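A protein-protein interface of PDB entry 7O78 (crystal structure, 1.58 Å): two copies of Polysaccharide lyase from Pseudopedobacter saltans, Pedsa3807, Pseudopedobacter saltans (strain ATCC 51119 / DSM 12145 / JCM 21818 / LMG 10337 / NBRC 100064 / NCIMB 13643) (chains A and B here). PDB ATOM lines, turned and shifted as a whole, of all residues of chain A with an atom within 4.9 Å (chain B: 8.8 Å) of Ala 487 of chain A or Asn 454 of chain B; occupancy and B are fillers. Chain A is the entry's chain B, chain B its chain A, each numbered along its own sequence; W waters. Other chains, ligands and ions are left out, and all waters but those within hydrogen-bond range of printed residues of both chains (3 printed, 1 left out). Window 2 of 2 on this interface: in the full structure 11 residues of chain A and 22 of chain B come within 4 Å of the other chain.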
ATOM      1  N   GLN A 483      16.735 -10.580   8.437  1.00  0.00           N
ATOM      2  CA  GLN A 483      17.161 -11.922   8.821  1.00  0.00           C
ATOM      3  C   GLN A 483      15.965 -12.880   8.926  1.00  0.00           C
ATOM      4  O   GLN A 483      16.101 -14.052   8.538  1.00  0.00           O
ATOM      5  CB  GLN A 483      17.982 -11.835  10.155  1.00  0.00           C
ATOM      6  CG  GLN A 483      19.132 -10.788  10.126  1.00  0.00           C
ATOM      7  CD  GLN A 483      19.899 -10.517  11.453  1.00  0.00           C
ATOM      8  OE1 GLN A 483      19.569  -9.566  12.201  1.00  0.00           O
ATOM      9  NE2 GLN A 483      20.966 -11.302  11.710  1.00  0.00           N
ATOM     10  N   ARG A 484      14.748 -12.381   9.325  1.00  0.00           N
ATOM     11  CA  ARG A 484      13.552 -13.238   9.316  1.00  0.00           C
ATOM     12  C   ARG A 484      13.173 -13.665   7.896  1.00  0.00           C
ATOM     13  O   ARG A 484      12.803 -14.823   7.657  1.00  0.00           O
ATOM     14  CB  ARG A 484      12.328 -12.533   9.943  1.00  0.00           C
ATOM     15  CG  ARG A 484      12.217 -12.468  11.431  1.00  0.00           C
ATOM     16  CD  ARG A 484      12.223 -13.890  12.134  1.00  0.00           C
ATOM     17  NE  ARG A 484      10.948 -14.518  12.550  1.00  0.00           N
ATOM     18  CZ  ARG A 484      10.266 -14.218  13.665  1.00  0.00           C
ATOM     19  NH1 ARG A 484      10.714 -13.295  14.515  1.00  0.00           N
ATOM     20  NH2 ARG A 484       9.135 -14.860  13.963  1.00  0.00           N
ATOM     21  N   VAL A 485      13.205 -12.721   6.947  1.00  0.00           N
ATOM     22  CA  VAL A 485      12.882 -13.041   5.561  1.00  0.00           C
ATOM     23  C   VAL A 485      13.822 -14.097   5.001  1.00  0.00           C
ATOM     24  O   VAL A 485      13.394 -15.068   4.365  1.00  0.00           O
ATOM     25  CB  VAL A 485      12.984 -11.751   4.713  1.00  0.00           C
ATOM     26  CG1 VAL A 485      12.884 -12.084   3.199  1.00  0.00           C
ATOM     27  CG2 VAL A 485      11.862 -10.768   5.133  1.00  0.00           C
ATOM     28  N   LEU A 486      15.108 -13.893   5.205  1.00  0.00           N
ATOM     29  CA  LEU A 486      16.114 -14.818   4.690  1.00  0.00           C
ATOM     30  C   LEU A 486      16.007 -16.210   5.322  1.00  0.00           C
ATOM     31  O   LEU A 486      16.179 -17.213   4.625  1.00  0.00           O
ATOM     32  CB  LEU A 486      17.507 -14.213   4.913  1.00  0.00           C
ATOM     33  CG  LEU A 486      17.702 -12.908   4.129  1.00  0.00           C
ATOM     34  CD1 LEU A 486      19.045 -12.311   4.581  1.00  0.00           C
ATOM     35  CD2 LEU A 486      17.688 -13.152   2.622  1.00  0.00           C
ATOM     36  N   ALA A 487      15.713 -16.299   6.635  1.00  0.00           N
ATOM     37  CA  ALA A 487      15.565 -17.614   7.278  1.00  0.00           C
ATOM     38  C   ALA A 487      14.322 -18.347   6.788  1.00  0.00           C
ATOM     39  O   ALA A 487      14.360 -19.565   6.578  1.00  0.00           O
ATOM     40  CB  ALA A 487      15.522 -17.449   8.790  1.00  0.00           C
ATOM     41  N   ARG A 488      13.213 -17.621   6.561  1.00  0.00           N
ATOM     42  CA  ARG A 488      12.015 -18.258   6.065  1.00  0.00           C
ATOM     43  C   ARG A 488      12.240 -18.798   4.661  1.00  0.00           C
ATOM     44  O   ARG A 488      11.729 -19.864   4.314  1.00  0.00           O
ATOM     45  CB  ARG A 488      10.840 -17.249   6.079  1.00  0.00           C
ATOM     46  CG  ARG A 488       9.437 -17.810   5.677  1.00  0.00           C
ATOM     47  CD  ARG A 488       8.274 -16.811   5.886  1.00  0.00           C
ATOM     48  NE  ARG A 488       7.096 -17.187   5.099  1.00  0.00           N
ATOM     49  CZ  ARG A 488       6.665 -16.539   4.005  1.00  0.00           C
ATOM     50  NH1 ARG A 488       7.327 -15.479   3.528  1.00  0.00           N
ATOM     51  NH2 ARG A 488       5.580 -16.982   3.380  1.00  0.00           N
ATOM     52  N   ASP A 489      12.984 -18.052   3.828  1.00  0.00           N
ATOM     53  CA  ASP A 489      13.319 -18.516   2.483  1.00  0.00           C
ATOM     54  C   ASP A 489      14.212 -19.756   2.519  1.00  0.00           C
ATOM     55  O   ASP A 489      13.950 -20.722   1.792  1.00  0.00           O
ATOM     56  CB  ASP A 489      14.009 -17.392   1.702  1.00  0.00           C
ATOM     57  CG  ASP A 489      14.524 -17.852   0.358  1.00  0.00           C
ATOM     58  OD1 ASP A 489      13.685 -17.999  -0.545  1.00  0.00           O
ATOM     59  OD2 ASP A 489      15.767 -18.012   0.203  1.00  0.00           O
ATOM     60  N   ARG A 490      15.284 -19.732   3.331  1.00  0.00           N
ATOM     61  CA  ARG A 490      16.216 -20.862   3.385  1.00  0.00           C
ATOM     62  C   ARG A 490      15.480 -22.138   3.764  1.00  0.00           C
ATOM     63  O   ARG A 490      15.780 -23.216   3.255  1.00  0.00           O
ATOM     64  CB  ARG A 490      17.337 -20.612   4.405  1.00  0.00           C
ATOM     65  CG  ARG A 490      18.460 -19.674   3.973  1.00  0.00           C
ATOM     66  CD  ARG A 490      19.689 -19.677   4.914  1.00  0.00           C
ATOM     67  NE  ARG A 490      19.413 -19.372   6.332  1.00  0.00           N
ATOM     68  CZ  ARG A 490      19.510 -18.153   6.877  1.00  0.00           C
ATOM     69  NH1 ARG A 490      19.820 -17.098   6.122  1.00  0.00           N
ATOM     70  NH2 ARG A 490      19.259 -17.975   8.167  1.00  0.00           N
ATOM     71  N   ASN A 491      14.468 -22.023   4.600  1.00  0.00           N
ATOM     72  CA  ASN A 491      13.739 -23.172   5.091  1.00  0.00           C
ATOM     73  C   ASN A 491      12.438 -23.445   4.329  1.00  0.00           C
ATOM     74  O   ASN A 491      11.715 -24.378   4.690  1.00  0.00           O
ATOM     75  CB  ASN A 491      13.502 -22.990   6.600  1.00  0.00           C
ATOM     76  CG  ASN A 491      14.799 -23.163   7.411  1.00  0.00           C
ATOM     77  OD1 ASN A 491      15.277 -24.301   7.575  1.00  0.00           O
ATOM     78  ND2 ASN A 491      15.411 -22.040   7.853  1.00  0.00           N
ATOM     79  N   HIS B 142      24.060 -16.294  15.994  1.00  0.00           N
ATOM     80  CA  HIS B 142      23.847 -17.605  15.384  1.00  0.00           C
ATOM     81  C   HIS B 142      24.671 -18.669  16.069  1.00  0.00           C
ATOM     82  O   HIS B 142      25.184 -19.586  15.436  1.00  0.00           O
ATOM     83  CB  HIS B 142      24.141 -17.537  13.887  1.00  0.00           C
ATOM     84  CG  HIS B 142      23.176 -16.641  13.172  1.00  0.00           C
ATOM     85  ND1 HIS B 142      23.413 -15.295  12.940  1.00  0.00           N
ATOM     86  CD2 HIS B 142      21.921 -16.890  12.717  1.00  0.00           C
ATOM     87  CE1 HIS B 142      22.350 -14.763  12.350  1.00  0.00           C
ATOM     88  NE2 HIS B 142      21.446 -15.714  12.158  1.00  0.00           N
ATOM     89  N   HIS B 180      20.143 -13.960  17.608  1.00  0.00           N
ATOM     90  CA  HIS B 180      19.909 -15.229  16.894  1.00  0.00           C
ATOM     91  C   HIS B 180      20.688 -16.375  17.537  1.00  0.00           C
ATOM     92  O   HIS B 180      21.234 -17.243  16.866  1.00  0.00           O
ATOM     93  CB  HIS B 180      20.274 -15.064  15.407  1.00  0.00           C
ATOM     94  CG  HIS B 180      19.414 -14.051  14.752  1.00  0.00           C
ATOM     95  ND1 HIS B 180      19.772 -12.712  14.648  1.00  0.00           N
ATOM     96  CD2 HIS B 180      18.167 -14.161  14.234  1.00  0.00           C
ATOM     97  CE1 HIS B 180      18.770 -12.046  14.060  1.00  0.00           C
ATOM     98  NE2 HIS B 180      17.790 -12.900  13.798  1.00  0.00           N
ATOM     99  N   PHE B 182      20.784 -19.665  20.449  1.00  0.00           N
ATOM    100  CA  PHE B 182      19.866 -20.642  21.013  1.00  0.00           C
ATOM    101  C   PHE B 182      20.419 -21.139  22.336  1.00  0.00           C
ATOM    102  O   PHE B 182      21.607 -21.452  22.409  1.00  0.00           O
ATOM    103  CB  PHE B 182      19.740 -21.825  20.064  1.00  0.00           C
ATOM    104  CG  PHE B 182      18.812 -22.920  20.609  1.00  0.00           C
ATOM    105  CD1 PHE B 182      17.455 -22.829  20.338  1.00  0.00           C
ATOM    106  CD2 PHE B 182      19.304 -23.995  21.308  1.00  0.00           C
ATOM    107  CE1 PHE B 182      16.559 -23.818  20.852  1.00  0.00           C
ATOM    108  CE2 PHE B 182      18.412 -24.984  21.817  1.00  0.00           C
ATOM    109  CZ  PHE B 182      17.061 -24.882  21.585  1.00  0.00           C
ATOM    110  N   LEU B 214      16.536 -17.304  21.111  1.00  0.00           N
ATOM    111  CA  LEU B 214      15.563 -18.331  21.458  1.00  0.00           C
ATOM    112  C   LEU B 214      16.082 -19.125  22.634  1.00  0.00           C
ATOM    113  O   LEU B 214      17.113 -19.804  22.526  1.00  0.00           O
ATOM    114  CB  LEU B 214      15.352 -19.248  20.245  1.00  0.00           C
ATOM    115  CG  LEU B 214      14.413 -20.420  20.455  1.00  0.00           C
ATOM    116  CD1 LEU B 214      13.012 -19.969  20.948  1.00  0.00           C
ATOM    117  CD2 LEU B 214      14.299 -21.216  19.183  1.00  0.00           C
ATOM    118  N   LEU B 451       9.815 -16.851  17.789  1.00  0.00           N
ATOM    119  CA  LEU B 451      10.867 -17.479  17.000  1.00  0.00           C
ATOM    120  C   LEU B 451      10.799 -19.012  17.137  1.00  0.00           C
ATOM    121  O   LEU B 451      10.388 -19.568  18.172  1.00  0.00           O
ATOM    122  CB  LEU B 451      12.249 -17.044  17.543  1.00  0.00           C
ATOM    123  CG  LEU B 451      12.517 -15.569  17.328  1.00  0.00           C
ATOM    124  CD1 LEU B 451      13.676 -15.194  18.305  1.00  0.00           C
ATOM    125  CD2 LEU B 451      12.931 -15.341  15.909  1.00  0.00           C
ATOM    126  N   THR B 452      11.244 -19.677  16.077  1.00  0.00           N
ATOM    127  CA  THR B 452      11.445 -21.125  16.057  1.00  0.00           C
ATOM    128  C   THR B 452      12.929 -21.394  15.829  1.00  0.00           C
ATOM    129  O   THR B 452      13.708 -20.488  15.520  1.00  0.00           O
ATOM    130  CB  THR B 452      10.612 -21.812  14.971  1.00  0.00           C
ATOM    131  OG1 THR B 452      11.145 -21.457  13.702  1.00  0.00           O
ATOM    132  CG2 THR B 452       9.139 -21.316  15.011  1.00  0.00           C
ATOM    133  N   TRP B 453      13.311 -22.655  15.981  1.00  0.00           N
ATOM    134  CA  TRP B 453      14.713 -23.058  15.771  1.00  0.00           C
ATOM    135  C   TRP B 453      15.230 -22.663  14.390  1.00  0.00           C
ATOM    136  O   TRP B 453      16.348 -22.145  14.275  1.00  0.00           O
ATOM    137  CB  TRP B 453      14.796 -24.600  15.967  1.00  0.00           C
ATOM    138  CG  TRP B 453      16.061 -25.276  15.485  1.00  0.00           C
ATOM    139  CD1 TRP B 453      16.108 -26.275  14.578  1.00  0.00           C
ATOM    140  CD2 TRP B 453      17.401 -25.078  15.957  1.00  0.00           C
ATOM    141  NE1 TRP B 453      17.412 -26.740  14.416  1.00  0.00           N
ATOM    142  CE2 TRP B 453      18.221 -26.024  15.275  1.00  0.00           C
ATOM    143  CE3 TRP B 453      17.998 -24.230  16.922  1.00  0.00           C
ATOM    144  CZ2 TRP B 453      19.569 -26.136  15.487  1.00  0.00           C
ATOM    145  CZ3 TRP B 453      19.382 -24.339  17.121  1.00  0.00           C
ATOM    146  CH2 TRP B 453      20.141 -25.299  16.425  1.00  0.00           C
ATOM    147  N   ASN B 454      14.415 -22.820  13.338  1.00  0.00           N
ATOM    148  CA  ASN B 454      14.889 -22.472  12.001  1.00  0.00           C
ATOM    149  C   ASN B 454      15.106 -20.979  11.812  1.00  0.00           C
ATOM    150  O   ASN B 454      15.840 -20.578  10.889  1.00  0.00           O
ATOM    151  CB  ASN B 454      13.909 -23.001  10.926  1.00  0.00           C
ATOM    152  CG  ASN B 454      13.989 -24.533  10.766  1.00  0.00           C
ATOM    153  OD1 ASN B 454      15.002 -25.160  11.004  1.00  0.00           O
ATOM    154  ND2 ASN B 454      12.863 -25.136  10.359  1.00  0.00           N
ATOM    155  N   ASP B 455      14.522 -20.143  12.683  1.00  0.00           N
ATOM    156  CA  ASP B 455      14.749 -18.701  12.646  1.00  0.00           C
ATOM    157  C   ASP B 455      16.094 -18.279  13.213  1.00  0.00           C
ATOM    158  O   ASP B 455      16.505 -17.145  12.953  1.00  0.00           O
ATOM    159  CB  ASP B 455      13.652 -17.960  13.405  1.00  0.00           C
ATOM    160  CG  ASP B 455      12.263 -18.141  12.775  1.00  0.00           C
ATOM    161  OD1 ASP B 455      12.162 -18.100  11.530  1.00  0.00           O
ATOM    162  OD2 ASP B 455      11.283 -18.323  13.507  1.00  0.00           O
ATOM    163  N   VAL B 456      16.769 -19.127  14.009  1.00  0.00           N
ATOM    164  CA  VAL B 456      18.006 -18.694  14.665  1.00  0.00           C
ATOM    165  C   VAL B 456      19.204 -19.562  14.315  1.00  0.00           C
ATOM    166  O   VAL B 456      20.340 -19.130  14.534  1.00  0.00           O
ATOM    167  CB  VAL B 456      17.853 -18.602  16.205  1.00  0.00           C
ATOM    168  CG1 VAL B 456      16.678 -17.660  16.566  1.00  0.00           C
ATOM    169  CG2 VAL B 456      17.579 -20.004  16.813  1.00  0.00           C
ATOM    170  N   ARG B 457      19.005 -20.813  13.872  1.00  0.00           N
ATOM    171  CA  ARG B 457      20.090 -21.771  13.795  1.00  0.00           C
ATOM    172  C   ARG B 457      21.155 -21.367  12.783  1.00  0.00           C
ATOM    173  O   ARG B 457      20.851 -20.719  11.772  1.00  0.00           O
ATOM    174  CB  ARG B 457      19.529 -23.161  13.450  1.00  0.00           C
ATOM    175  CG  ARG B 457      18.970 -23.239  12.047  1.00  0.00           C
ATOM    176  CD  ARG B 457      18.321 -24.622  11.850  1.00  0.00           C
ATOM    177  NE  ARG B 457      17.727 -24.674  10.500  1.00  0.00           N
ATOM    178  CZ  ARG B 457      18.418 -25.006   9.413  1.00  0.00           C
ATOM    179  NH1 ARG B 457      19.687 -25.302   9.480  1.00  0.00           N
ATOM    180  NH2 ARG B 457      17.850 -25.029   8.216  1.00  0.00           N
ATOM    181  N   PRO B 458      22.397 -21.835  12.997  1.00  0.00           N
ATOM    182  CA  PRO B 458      23.445 -21.743  11.965  1.00  0.00           C
ATOM    183  C   PRO B 458      22.959 -22.464  10.730  1.00  0.00           C
ATOM    184  O   PRO B 458      22.325 -23.493  10.864  1.00  0.00           O
ATOM    185  CB  PRO B 458      24.630 -22.493  12.593  1.00  0.00           C
ATOM    186  CG  PRO B 458      24.348 -22.503  14.039  1.00  0.00           C
ATOM    187  CD  PRO B 458      22.866 -22.592  14.164  1.00  0.00           C
ATOM    188  N   SER B 459      23.183 -21.882   9.547  1.00  0.00           N
ATOM    189  CA  SER B 459      22.580 -22.487   8.370  1.00  0.00           C
ATOM    190  C   SER B 459      23.058 -23.915   8.147  1.00  0.00           C
ATOM    191  O   SER B 459      22.332 -24.716   7.565  1.00  0.00           O
ATOM    192  CB  SER B 459      22.890 -21.624   7.139  1.00  0.00           C
ATOM    193  OG  SER B 459      24.301 -21.503   7.060  1.00  0.00           O
ATOM    194  N   LEU B 461      23.593 -26.271  10.520  1.00  0.00           N
ATOM    195  CA  LEU B 461      23.227 -27.191  11.594  1.00  0.00           C
ATOM    196  C   LEU B 461      21.733 -27.436  11.529  1.00  0.00           C
ATOM    197  O   LEU B 461      20.948 -26.541  11.862  1.00  0.00           O
ATOM    198  CB  LEU B 461      23.608 -26.571  12.951  1.00  0.00           C
ATOM    199  CG  LEU B 461      23.245 -27.465  14.142  1.00  0.00           C
ATOM    200  CD1 LEU B 461      24.111 -28.723  14.159  1.00  0.00           C
ATOM    201  CD2 LEU B 461      23.441 -26.665  15.473  1.00  0.00           C
ATOM    202  N   VAL B 462      21.333 -28.689  11.243  1.00  0.00           N
ATOM    203  CA  VAL B 462      19.914 -28.967  11.025  1.00  0.00           C
ATOM    204  C   VAL B 462      19.169 -29.147  12.335  1.00  0.00           C
ATOM    205  O   VAL B 462      18.039 -28.669  12.468  1.00  0.00           O
ATOM    206  CB  VAL B 462      19.740 -30.208  10.124  1.00  0.00           C
ATOM    207  CG1 VAL B 462      18.248 -30.502   9.900  1.00  0.00           C
ATOM    208  CG2 VAL B 462      20.403 -29.964   8.806  1.00  0.00           C
ATOM    209  N   GLU B 463      19.732 -29.901  13.269  1.00  0.00           N
ATOM    210  CA  GLU B 463      19.008 -30.264  14.479  1.00  0.00           C
ATOM    211  C   GLU B 463      19.672 -29.682  15.715  1.00  0.00           C
ATOM    212  O   GLU B 463      20.892 -29.527  15.778  1.00  0.00           O
ATOM    213  CB  GLU B 463      18.951 -31.797  14.640  1.00  0.00           C
ATOM    214  N   ILE B 464      18.850 -29.406  16.722  1.00  0.00           N
ATOM    215  CA  ILE B 464      19.360 -28.929  18.004  1.00  0.00           C
ATOM    216  C   ILE B 464      20.295 -29.969  18.594  1.00  0.00           C
ATOM    217  O   ILE B 464      19.901 -31.149  18.731  1.00  0.00           O
ATOM    218  CB  ILE B 464      18.175 -28.680  18.951  1.00  0.00           C
ATOM    219  CG1 ILE B 464      17.265 -27.593  18.408  1.00  0.00           C
ATOM    220  CG2 ILE B 464      18.667 -28.358  20.372  1.00  0.00           C
ATOM    221  CD1 ILE B 464      15.913 -27.498  19.170  1.00  0.00           C
HETATM  222  O   HOH W   1      18.968 -19.574  10.399  1.00  0.00           O
HETATM  223  O   HOH W   2       8.728 -17.597  13.304  1.00  0.00           O
HETATM  224  O   HOH W   3      15.339 -14.875  11.707  1.00  0.00           O
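The side-chain carboxylate (OD1) of Asp 455 of chain B is in salt-bridge range of the guanidinium group (NE) of Arg 484 of chain A, at 3.9 Å.
The backbone carbonyl oxygen (O) of Asn 454 of chain B lies within hydrogen-bond range of the side-chain amide nitrogen (ND2) of Asn 491 of chain A (3.4 Å).
NE2 of Gln 483 of chain A sits close to ND1 of His 180 of chain B, 3.5 Å away.
NH2 of Arg 457 of chain B lies within hydrogen-bond range of OD1 of Asn 491 of chain A (2.7 Å).
Of the printed residues of chain B, Gln 483 of chain A touches His 142 (3.8 Å) and His 180 (3.2 Å).
Printed residues of chain B within 4 Å of Arg 484 of chain A: Leu 451 (3.3 Å) and Asp 455 (3.9 Å).
Leu 486 of chain A touches none of the printed residues of chain B.
Ala 487 of chain A touches just one residue of chain B: Asn 454.
Of the printed residues of chain A, Leu 451 of chain B touches Arg 484 (3.3 Å).
Printed residues of chain A within 4 Å of Asn 454 of chain B: Ala 487 (3.8 Å) and Asn 491 (3.4 Å).
Printed residues of chain A within 4 Å of Asp 455 of chain B: Arg 484 (3.9 Å).
Of the printed residues of chain A, Arg 457 of chain B touches Asn 491.
Ser 459 of chain B touches none of the printed residues of chain A.
Among the printed residues, merely in contact across the chains: Gln 483 of chain A with His 142 of chain B (3.8 Å), Arg 484 of chain A with Leu 451 of chain B (3.3 Å) and Ala 487 of chain A with Asn 454 of chain B (3.8 Å).
Water W1 lies within hydrogen-bond range of the backbone carbonyl oxygen of Arg 457 of chain B (2.6 Å), the guanidinium group of Arg 490 of chain A (2.8 Å) and the backbone carbonyl oxygen of Asn 454 of chain B (3.3 Å).
Water W2 bridges OD2 of Asp 455 of chain B (2.7 Å) and NH2 of Arg 484 of chain A (2.8 Å).
Water W3 lies within hydrogen-bond range of the backbone carbonyl oxygen (O) of Asp 455 of chain B (2.8 Å), the backbone carbonyl oxygen (O) of Gln 483 of chain A (3.4 Å) and the backbone NH (N) of Arg 484 of chain A (3.5 Å).
The backbone carbonyl oxygen (O) of Leu 461 of chain B lies within hydrogen-bond range of the guanidinium group (NH1) of Arg 457 of chain B (3.0 Å).
The side-chain amide oxygen (OD1) of Asn 454 of chain B is in hydrogen-bond range of the guanidinium group (NE) of Arg 457 of chain B (2.8 Å).
O of His 180 of chain B lies close to N of His 142 of chain B, 3.1 Å away.
The backbone NH (N) of Thr 452 of chain B lies within hydrogen-bond range of the side-chain carboxylate (OD2) of Asp 455 of chain B (2.9 Å).
NH1 of Arg 457 of chain B is in hydrogen-bond range of O of Ser 459 of chain B, 3.3 Å away.
O of Ala 487 of chain A sits at hydrogen-bond distance from ND2 of Asn 491 of chain A (3.0 Å).
No position is printed for both chains.
Of the 9 printed residues of chain A, 4 touch a printed residue of chain B.
Along chain A the printed residues that touch a printed residue of chain B span positions 483 to 491.
Printed residues of chain B that touch a printed residue of chain A: His 142, His 180, Leu 451, Asn 454, Asp 455 and Arg 457.
Hydrophobic or aromatic side chains of chain B within 4 Å of the printed part of chain A: His 142, His 180 and Leu 451.
Among the printed residues, Asp or Glu carboxylates within 4 Å of a Lys or Arg side-chain nitrogen of the other chain: Arg 484 of chain A with Asp 455 of chain B.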
